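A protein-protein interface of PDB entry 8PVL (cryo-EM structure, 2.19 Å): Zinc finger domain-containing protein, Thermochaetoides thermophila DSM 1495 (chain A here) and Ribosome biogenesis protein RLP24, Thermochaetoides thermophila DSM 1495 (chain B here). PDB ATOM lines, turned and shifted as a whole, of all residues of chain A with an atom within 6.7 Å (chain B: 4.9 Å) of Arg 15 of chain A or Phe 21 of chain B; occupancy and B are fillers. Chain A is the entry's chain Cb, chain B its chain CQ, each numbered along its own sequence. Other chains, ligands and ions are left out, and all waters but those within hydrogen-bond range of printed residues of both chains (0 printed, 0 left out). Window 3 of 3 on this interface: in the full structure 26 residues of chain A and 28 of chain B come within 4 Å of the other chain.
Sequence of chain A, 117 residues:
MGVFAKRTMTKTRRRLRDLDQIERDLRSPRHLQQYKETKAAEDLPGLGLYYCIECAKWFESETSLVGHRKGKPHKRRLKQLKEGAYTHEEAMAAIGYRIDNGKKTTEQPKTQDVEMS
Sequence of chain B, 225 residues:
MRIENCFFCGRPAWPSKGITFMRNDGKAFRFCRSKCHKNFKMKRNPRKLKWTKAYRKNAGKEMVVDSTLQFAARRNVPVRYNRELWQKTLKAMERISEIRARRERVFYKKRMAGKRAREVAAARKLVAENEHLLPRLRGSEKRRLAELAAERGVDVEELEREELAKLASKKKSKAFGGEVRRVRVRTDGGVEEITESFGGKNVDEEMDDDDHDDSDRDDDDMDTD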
ATOM      1  N   MET A   9     -11.626  10.307  -0.439  1.00  0.00           N
ATOM      2  CA  MET A   9     -12.888  11.028  -0.295  1.00  0.00           C
ATOM      3  C   MET A   9     -13.005  11.711   1.059  1.00  0.00           C
ATOM      4  O   MET A   9     -13.646  12.761   1.168  1.00  0.00           O
ATOM      5  CB  MET A   9     -14.071  10.080  -0.480  1.00  0.00           C
ATOM      6  CG  MET A   9     -15.336  10.766  -0.969  1.00  0.00           C
ATOM      7  SD  MET A   9     -16.806   9.715  -1.019  1.00  0.00           S
ATOM      8  CE  MET A   9     -16.141   8.103  -0.615  1.00  0.00           C
ATOM      9  N   THR A  10     -12.414  11.130   2.098  1.00  0.00           N
ATOM     10  CA  THR A  10     -12.581  11.615   3.459  1.00  0.00           C
ATOM     11  C   THR A  10     -11.511  12.614   3.878  1.00  0.00           C
ATOM     12  O   THR A  10     -11.513  13.046   5.033  1.00  0.00           O
ATOM     13  CB  THR A  10     -12.597  10.439   4.441  1.00  0.00           C
ATOM     14  OG1 THR A  10     -11.386   9.686   4.314  1.00  0.00           O
ATOM     15  CG2 THR A  10     -13.785   9.529   4.164  1.00  0.00           C
ATOM     16  N   LYS A  11     -10.602  12.986   2.981  1.00  0.00           N
ATOM     17  CA  LYS A  11      -9.622  14.014   3.296  1.00  0.00           C
ATOM     18  C   LYS A  11     -10.306  15.365   3.477  1.00  0.00           C
ATOM     19  O   LYS A  11     -11.360  15.633   2.894  1.00  0.00           O
ATOM     20  CB  LYS A  11      -8.562  14.111   2.198  1.00  0.00           C
ATOM     21  CG  LYS A  11      -7.425  13.111   2.327  1.00  0.00           C
ATOM     22  CD  LYS A  11      -6.338  13.377   1.293  1.00  0.00           C
ATOM     23  CE  LYS A  11      -5.084  12.563   1.565  1.00  0.00           C
ATOM     24  NZ  LYS A  11      -4.302  13.079   2.719  1.00  0.00           N
ATOM     25  N   THR A  12      -9.703  16.209   4.318  1.00  0.00           N
ATOM     26  CA  THR A  12     -10.251  17.539   4.571  1.00  0.00           C
ATOM     27  C   THR A  12     -10.212  18.408   3.318  1.00  0.00           C
ATOM     28  O   THR A  12     -11.094  19.249   3.117  1.00  0.00           O
ATOM     29  CB  THR A  12      -9.485  18.205   5.717  1.00  0.00           C
ATOM     30  OG1 THR A  12      -9.377  17.289   6.814  1.00  0.00           O
ATOM     31  CG2 THR A  12     -10.202  19.458   6.202  1.00  0.00           C
ATOM     32  N   ARG A  13      -9.223  18.196   2.448  1.00  0.00           N
ATOM     33  CA  ARG A  13      -9.121  18.955   1.207  1.00  0.00           C
ATOM     34  C   ARG A  13     -10.126  18.510   0.150  1.00  0.00           C
ATOM     35  O   ARG A  13     -10.173  19.122  -0.922  1.00  0.00           O
ATOM     36  CB  ARG A  13      -7.696  18.868   0.655  1.00  0.00           C
ATOM     37  CG  ARG A  13      -7.261  17.490   0.186  1.00  0.00           C
ATOM     38  CD  ARG A  13      -6.022  17.596  -0.686  1.00  0.00           C
ATOM     39  NE  ARG A  13      -5.326  16.325  -0.847  1.00  0.00           N
ATOM     40  CZ  ARG A  13      -5.601  15.430  -1.786  1.00  0.00           C
ATOM     41  NH1 ARG A  13      -6.577  15.619  -2.657  1.00  0.00           N
ATOM     42  NH2 ARG A  13      -4.879  14.316  -1.850  1.00  0.00           N
ATOM     43  N   ARG A  14     -10.917  17.469   0.415  1.00  0.00           N
ATOM     44  CA  ARG A  14     -11.999  17.042  -0.465  1.00  0.00           C
ATOM     45  C   ARG A  14     -13.368  17.206   0.186  1.00  0.00           C
ATOM     46  O   ARG A  14     -14.344  16.606  -0.273  1.00  0.00           O
ATOM     47  CB  ARG A  14     -11.795  15.589  -0.893  1.00  0.00           C
ATOM     48  CG  ARG A  14     -10.483  15.319  -1.602  1.00  0.00           C
ATOM     49  CD  ARG A  14     -10.660  15.320  -3.107  1.00  0.00           C
ATOM     50  NE  ARG A  14     -11.787  14.495  -3.525  1.00  0.00           N
ATOM     51  CZ  ARG A  14     -11.733  13.183  -3.703  1.00  0.00           C
ATOM     52  NH1 ARG A  14     -10.616  12.504  -3.509  1.00  0.00           N
ATOM     53  NH2 ARG A  14     -12.830  12.536  -4.085  1.00  0.00           N
ATOM     54  N   ARG A  15     -13.457  18.004   1.247  1.00  0.00           N
ATOM     55  CA  ARG A  15     -14.689  18.116   2.018  1.00  0.00           C
ATOM     56  C   ARG A  15     -15.753  18.902   1.258  1.00  0.00           C
ATOM     57  O   ARG A  15     -15.462  19.914   0.614  1.00  0.00           O
ATOM     58  CB  ARG A  15     -14.398  18.786   3.362  1.00  0.00           C
ATOM     59  CG  ARG A  15     -15.601  18.928   4.272  1.00  0.00           C
ATOM     60  CD  ARG A  15     -15.335  19.901   5.402  1.00  0.00           C
ATOM     61  NE  ARG A  15     -16.577  20.387   5.990  1.00  0.00           N
ATOM     62  CZ  ARG A  15     -17.241  21.451   5.560  1.00  0.00           C
ATOM     63  NH1 ARG A  15     -16.808  22.169   4.538  1.00  0.00           N
ATOM     64  NH2 ARG A  15     -18.367  21.804   6.172  1.00  0.00           N
ATOM     65  N   LEU A  16     -16.993  18.428   1.338  1.00  0.00           N
ATOM     66  CA  LEU A  16     -18.143  19.078   0.727  1.00  0.00           C
ATOM     67  C   LEU A  16     -18.937  19.866   1.768  1.00  0.00           C
ATOM     68  O   LEU A  16     -18.734  19.737   2.976  1.00  0.00           O
ATOM     69  CB  LEU A  16     -19.040  18.044   0.040  1.00  0.00           C
ATOM     70  CG  LEU A  16     -18.374  17.183  -1.035  1.00  0.00           C
ATOM     71  CD1 LEU A  16     -19.374  16.220  -1.646  1.00  0.00           C
ATOM     72  CD2 LEU A  16     -17.744  18.053  -2.109  1.00  0.00           C
ATOM     73  N   ARG A  17     -19.855  20.694   1.271  1.00  0.00           N
ATOM     74  CA  ARG A  17     -20.647  21.566   2.131  1.00  0.00           C
ATOM     75  C   ARG A  17     -21.647  20.767   2.962  1.00  0.00           C
ATOM     76  O   ARG A  17     -22.262  19.812   2.479  1.00  0.00           O
ATOM     77  CB  ARG A  17     -21.376  22.609   1.285  1.00  0.00           C
ATOM     78  CG  ARG A  17     -21.958  23.767   2.071  1.00  0.00           C
ATOM     79  CD  ARG A  17     -22.115  24.998   1.192  1.00  0.00           C
ATOM     80  NE  ARG A  17     -22.727  26.116   1.901  1.00  0.00           N
ATOM     81  CZ  ARG A  17     -22.087  26.912   2.746  1.00  0.00           C
ATOM     82  NH1 ARG A  17     -20.804  26.745   3.019  1.00  0.00           N
ATOM     83  NH2 ARG A  17     -22.751  27.905   3.329  1.00  0.00           N
ATOM     84  N   ASP A  18     -21.812  21.171   4.219  1.00  0.00           N
ATOM     85  CA  ASP A  18     -22.649  20.453   5.168  1.00  0.00           C
ATOM     86  C   ASP A  18     -24.134  20.765   4.975  1.00  0.00           C
ATOM     87  O   ASP A  18     -24.528  21.808   4.437  1.00  0.00           O
ATOM     88  CB  ASP A  18     -22.238  20.776   6.604  1.00  0.00           C
ATOM     89  CG  ASP A  18     -20.946  20.098   7.007  1.00  0.00           C
ATOM     90  OD1 ASP A  18     -20.726  18.944   6.589  1.00  0.00           O
ATOM     91  OD2 ASP A  18     -20.149  20.716   7.746  1.00  0.00           O
ATOM     92  N   GLN A  21     -25.448  23.889   6.830  1.00  0.00           N
ATOM     93  CA  GLN A  21     -25.091  25.069   6.049  1.00  0.00           C
ATOM     94  C   GLN A  21     -26.008  25.227   4.843  1.00  0.00           C
ATOM     95  O   GLN A  21     -26.392  26.347   4.489  1.00  0.00           O
ATOM     96  CB  GLN A  21     -23.632  24.984   5.604  1.00  0.00           C
ATOM     97  CG  GLN A  21     -22.634  24.914   6.743  1.00  0.00           C
ATOM     98  CD  GLN A  21     -21.201  24.881   6.256  1.00  0.00           C
ATOM     99  OE1 GLN A  21     -20.753  23.893   5.678  1.00  0.00           O
ATOM    100  NE2 GLN A  21     -20.473  25.966   6.486  1.00  0.00           N
ATOM    101  N   ILE B  19     -11.584  15.117  19.578  1.00  0.00           N
ATOM    102  CA  ILE B  19     -11.031  16.099  18.651  1.00  0.00           C
ATOM    103  C   ILE B  19     -12.108  17.124  18.318  1.00  0.00           C
ATOM    104  O   ILE B  19     -13.305  16.834  18.358  1.00  0.00           O
ATOM    105  CB  ILE B  19     -10.464  15.400  17.386  1.00  0.00           C
ATOM    106  CG1 ILE B  19      -9.520  16.322  16.607  1.00  0.00           C
ATOM    107  CG2 ILE B  19     -11.577  14.858  16.494  1.00  0.00           C
ATOM    108  CD1 ILE B  19      -8.778  15.630  15.493  1.00  0.00           C
ATOM    109  N   THR B  20     -11.679  18.345  18.013  1.00  0.00           N
ATOM    110  CA  THR B  20     -12.591  19.436  17.708  1.00  0.00           C
ATOM    111  C   THR B  20     -12.409  19.869  16.260  1.00  0.00           C
ATOM    112  O   THR B  20     -11.279  20.048  15.796  1.00  0.00           O
ATOM    113  CB  THR B  20     -12.363  20.621  18.649  1.00  0.00           C
ATOM    114  OG1 THR B  20     -12.276  20.146  19.996  1.00  0.00           O
ATOM    115  CG2 THR B  20     -13.525  21.588  18.555  1.00  0.00           C
ATOM    116  N   PHE B  21     -13.519  20.026  15.552  1.00  0.00           N
ATOM    117  CA  PHE B  21     -13.520  20.497  14.174  1.00  0.00           C
ATOM    118  C   PHE B  21     -13.960  21.956  14.164  1.00  0.00           C
ATOM    119  O   PHE B  21     -15.044  22.285  14.654  1.00  0.00           O
ATOM    120  CB  PHE B  21     -14.445  19.644  13.306  1.00  0.00           C
ATOM    121  CG  PHE B  21     -14.687  20.208  11.934  1.00  0.00           C
ATOM    122  CD1 PHE B  21     -13.626  20.537  11.106  1.00  0.00           C
ATOM    123  CD2 PHE B  21     -15.976  20.404  11.471  1.00  0.00           C
ATOM    124  CE1 PHE B  21     -13.848  21.050   9.844  1.00  0.00           C
ATOM    125  CE2 PHE B  21     -16.203  20.917  10.209  1.00  0.00           C
ATOM    126  CZ  PHE B  21     -15.138  21.241   9.396  1.00  0.00           C
ATOM    127  N   MET B  22     -13.115  22.820  13.616  1.00  0.00           N
ATOM    128  CA  MET B  22     -13.380  24.252  13.545  1.00  0.00           C
ATOM    129  C   MET B  22     -13.854  24.544  12.126  1.00  0.00           C
ATOM    130  O   MET B  22     -13.082  24.395  11.174  1.00  0.00           O
ATOM    131  CB  MET B  22     -12.117  25.048  13.859  1.00  0.00           C
ATOM    132  CG  MET B  22     -11.640  25.057  15.310  1.00  0.00           C
ATOM    133  SD  MET B  22     -12.814  25.410  16.622  1.00  0.00           S
ATOM    134  CE  MET B  22     -11.891  24.827  18.026  1.00  0.00           C
ATOM    135  N   ARG B  23     -15.110  24.959  11.967  1.00  0.00           N
ATOM    136  CA  ARG B  23     -15.643  25.231  10.640  1.00  0.00           C
ATOM    137  C   ARG B  23     -15.538  26.718  10.318  1.00  0.00           C
ATOM    138  O   ARG B  23     -15.511  27.568  11.211  1.00  0.00           O
ATOM    139  CB  ARG B  23     -17.097  24.762  10.535  1.00  0.00           C
ATOM    140  CG  ARG B  23     -17.531  24.392   9.124  1.00  0.00           C
ATOM    141  CD  ARG B  23     -18.847  23.638   9.120  1.00  0.00           C
ATOM    142  NE  ARG B  23     -19.927  24.425   9.698  1.00  0.00           N
ATOM    143  CZ  ARG B  23     -21.165  23.986   9.867  1.00  0.00           C
ATOM    144  NH1 ARG B  23     -21.518  22.762   9.514  1.00  0.00           N
ATOM    145  NH2 ARG B  23     -22.073  24.796  10.403  1.00  0.00           N
ATOM    146  N   LYS B  27     -18.314  27.773  13.671  1.00  0.00           N
ATOM    147  CA  LYS B  27     -18.911  26.771  14.545  1.00  0.00           C
ATOM    148  C   LYS B  27     -17.895  25.690  14.886  1.00  0.00           C
ATOM    149  O   LYS B  27     -17.181  25.193  14.008  1.00  0.00           O
ATOM    150  CB  LYS B  27     -20.152  26.159  13.891  1.00  0.00           C
ATOM    151  CG  LYS B  27     -21.456  26.684  14.469  1.00  0.00           C
ATOM    152  CD  LYS B  27     -22.634  26.375  13.563  1.00  0.00           C
ATOM    153  CE  LYS B  27     -23.799  27.310  13.842  1.00  0.00           C
ATOM    154  NZ  LYS B  27     -23.450  28.731  13.561  1.00  0.00           N
ATOM    155  N   ALA B  28     -17.829  25.333  16.165  1.00  0.00           N
ATOM    156  CA  ALA B  28     -16.943  24.288  16.649  1.00  0.00           C
ATOM    157  C   ALA B  28     -17.738  23.020  16.928  1.00  0.00           C
ATOM    158  O   ALA B  28     -18.854  23.080  17.451  1.00  0.00           O
ATOM    159  CB  ALA B  28     -16.210  24.737  17.913  1.00  0.00           C
ATOM    160  N   PHE B  29     -17.158  21.875  16.577  1.00  0.00           N
ATOM    161  CA  PHE B  29     -17.796  20.574  16.756  1.00  0.00           C
ATOM    162  C   PHE B  29     -16.862  19.696  17.576  1.00  0.00           C
ATOM    163  O   PHE B  29     -15.821  19.264  17.077  1.00  0.00           O
ATOM    164  CB  PHE B  29     -18.104  19.915  15.409  1.00  0.00           C
ATOM    165  CG  PHE B  29     -19.064  20.689  14.553  1.00  0.00           C
ATOM    166  CD1 PHE B  29     -18.614  21.706  13.724  1.00  0.00           C
ATOM    167  CD2 PHE B  29     -20.415  20.389  14.566  1.00  0.00           C
ATOM    168  CE1 PHE B  29     -19.497  22.414  12.936  1.00  0.00           C
ATOM    169  CE2 PHE B  29     -21.302  21.094  13.778  1.00  0.00           C
ATOM    170  CZ  PHE B  29     -20.841  22.108  12.962  1.00  0.00           C
ATOM    171  N   PHE B  31     -15.954  16.254  19.321  1.00  0.00           N
ATOM    172  CA  PHE B  31     -16.224  14.828  19.263  1.00  0.00           C
ATOM    173  C   PHE B  31     -15.421  14.127  20.345  1.00  0.00           C
ATOM    174  O   PHE B  31     -14.256  14.462  20.579  1.00  0.00           O
ATOM    175  CB  PHE B  31     -15.859  14.246  17.897  1.00  0.00           C
ATOM    176  CG  PHE B  31     -16.448  14.997  16.750  1.00  0.00           C
ATOM    177  CD1 PHE B  31     -17.765  14.791  16.377  1.00  0.00           C
ATOM    178  CD2 PHE B  31     -15.691  15.917  16.047  1.00  0.00           C
ATOM    179  CE1 PHE B  31     -18.311  15.488  15.325  1.00  0.00           C
ATOM    180  CE2 PHE B  31     -16.231  16.616  14.997  1.00  0.00           C
ATOM    181  CZ  PHE B  31     -17.541  16.403  14.637  1.00  0.00           C
ATOM    182  N   PHE B  40     -18.902  11.574  11.352  1.00  0.00           N
ATOM    183  CA  PHE B  40     -19.188  12.951  10.964  1.00  0.00           C
ATOM    184  C   PHE B  40     -18.546  13.294   9.625  1.00  0.00           C
ATOM    185  O   PHE B  40     -19.172  13.933   8.772  1.00  0.00           O
ATOM    186  CB  PHE B  40     -18.697  13.901  12.054  1.00  0.00           C
ATOM    187  CG  PHE B  40     -18.960  15.352  11.767  1.00  0.00           C
ATOM    188  CD1 PHE B  40     -20.193  15.914  12.052  1.00  0.00           C
ATOM    189  CD2 PHE B  40     -17.965  16.161  11.235  1.00  0.00           C
ATOM    190  CE1 PHE B  40     -20.432  17.249  11.801  1.00  0.00           C
ATOM    191  CE2 PHE B  40     -18.201  17.496  10.985  1.00  0.00           C
ATOM    192  CZ  PHE B  40     -19.436  18.039  11.267  1.00  0.00           C
ATOM    193  N   LYS B  43     -20.378  12.003   6.934  1.00  0.00           N
ATOM    194  CA  LYS B  43     -21.672  12.696   6.854  1.00  0.00           C
ATOM    195  C   LYS B  43     -22.838  11.764   7.164  1.00  0.00           C
ATOM    196  O   LYS B  43     -23.910  11.879   6.568  1.00  0.00           O
ATOM    197  CB  LYS B  43     -21.907  13.388   5.497  1.00  0.00           C
ATOM    198  CG  LYS B  43     -20.727  14.149   4.907  1.00  0.00           C
ATOM    199  CD  LYS B  43     -20.669  15.589   5.373  1.00  0.00           C
ATOM    200  CE  LYS B  43     -19.639  16.364   4.564  1.00  0.00           C
ATOM    201  NZ  LYS B  43     -19.746  17.834   4.750  1.00  0.00           N
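The backbone NH of Phe 21 of chain B sits at hydrogen-bond distance from the backbone carbonyl oxygen of Phe 29 of chain B, at 2.9 Å.
The guanidinium group of Arg 15 of chain A is in hydrogen-bond range of the side-chain amide oxygen of Gln 21 of chain A (3.2 Å).
The guanidinium group (NH2) of Arg 15 of chain A is in salt-bridge range of the side-chain carboxylate (OD2) of Asp 18 of chain A, 2.6 Å away.
The backbone NH of Asp 18 of chain A lies within hydrogen-bond range of the side-chain amide oxygen of Gln 21 of chain A (3.3 Å).
Lys 11 of chain A touches none of the printed residues of chain B.
Of the printed residues of chain B, Arg 15 of chain A touches Phe 21 (3.8 Å) and Arg 23 (3.5 Å).
Of the printed residues of chain B, Leu 16 of chain A touches Lys 43.
Of the printed residues of chain B, Asp 18 of chain A touches Arg 23 (3.0 Å) and Lys 43 (2.4 Å).
Printed residues of chain B within 4 Å of Gln 21 of chain A: Arg 23.
Thr 20 of chain B touches none of the printed residues of chain A.
Of chain A, only Arg 15 comes within 4 Å of Phe 21 of chain B.
Of the printed residues of chain A, Lys 43 of chain B touches Leu 16 (2.8 Å), Arg 17 (3.9 Å) and Asp 18 (2.4 Å).
The nearest residue of chain B that does not touch Arg 15 of chain A is Lys 43 of chain B (4.3 Å).
The nearest residue of chain A that does not touch Phe 21 of chain B is Asp 18 of chain A (4.7 Å).
Among the printed residues, pairs that only touch across the chains: Arg 15 of chain A with Arg 23 of chain B (3.5 Å), Gln 21 of chain A with Arg 23 of chain B (3.6 Å), Arg 15 of chain A with Phe 21 of chain B (3.8 Å) and Arg 17 of chain A with Lys 43 of chain B (3.9 Å).
OD1 of Asp 18 of chain A sits close to NZ of Lys 43 of chain B (2.4 Å).
The guanidinium group (NH1) of Arg 23 of chain B lies within salt-bridge range of the side-chain carboxylate (OD2) of Asp 18 of chain A.
The side-chain amino group (NZ) of Lys 43 of chain B lies within hydrogen-bond range of the backbone carbonyl oxygen (O) of Leu 16 of chain A (2.8 Å).
Printed residues of chain A that touch a printed residue of chain B: Arg 15, Leu 16, Arg 17, Asp 18 and Gln 21.
Of the 11 printed residues of chain B, 3 touch a printed residue of chain A.
Hydrophobic or aromatic side chains of chain B that line the printed part of chain A: Phe 21.
Among the printed residues, Asp or Glu carboxylates within 4 Å of a Lys or Arg side-chain nitrogen of the other chain: Asp 18 of chain A with Arg 23 of chain B (3.0 Å) and Asp 18 of chain A with Lys 43 of chain B (2.4 Å).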
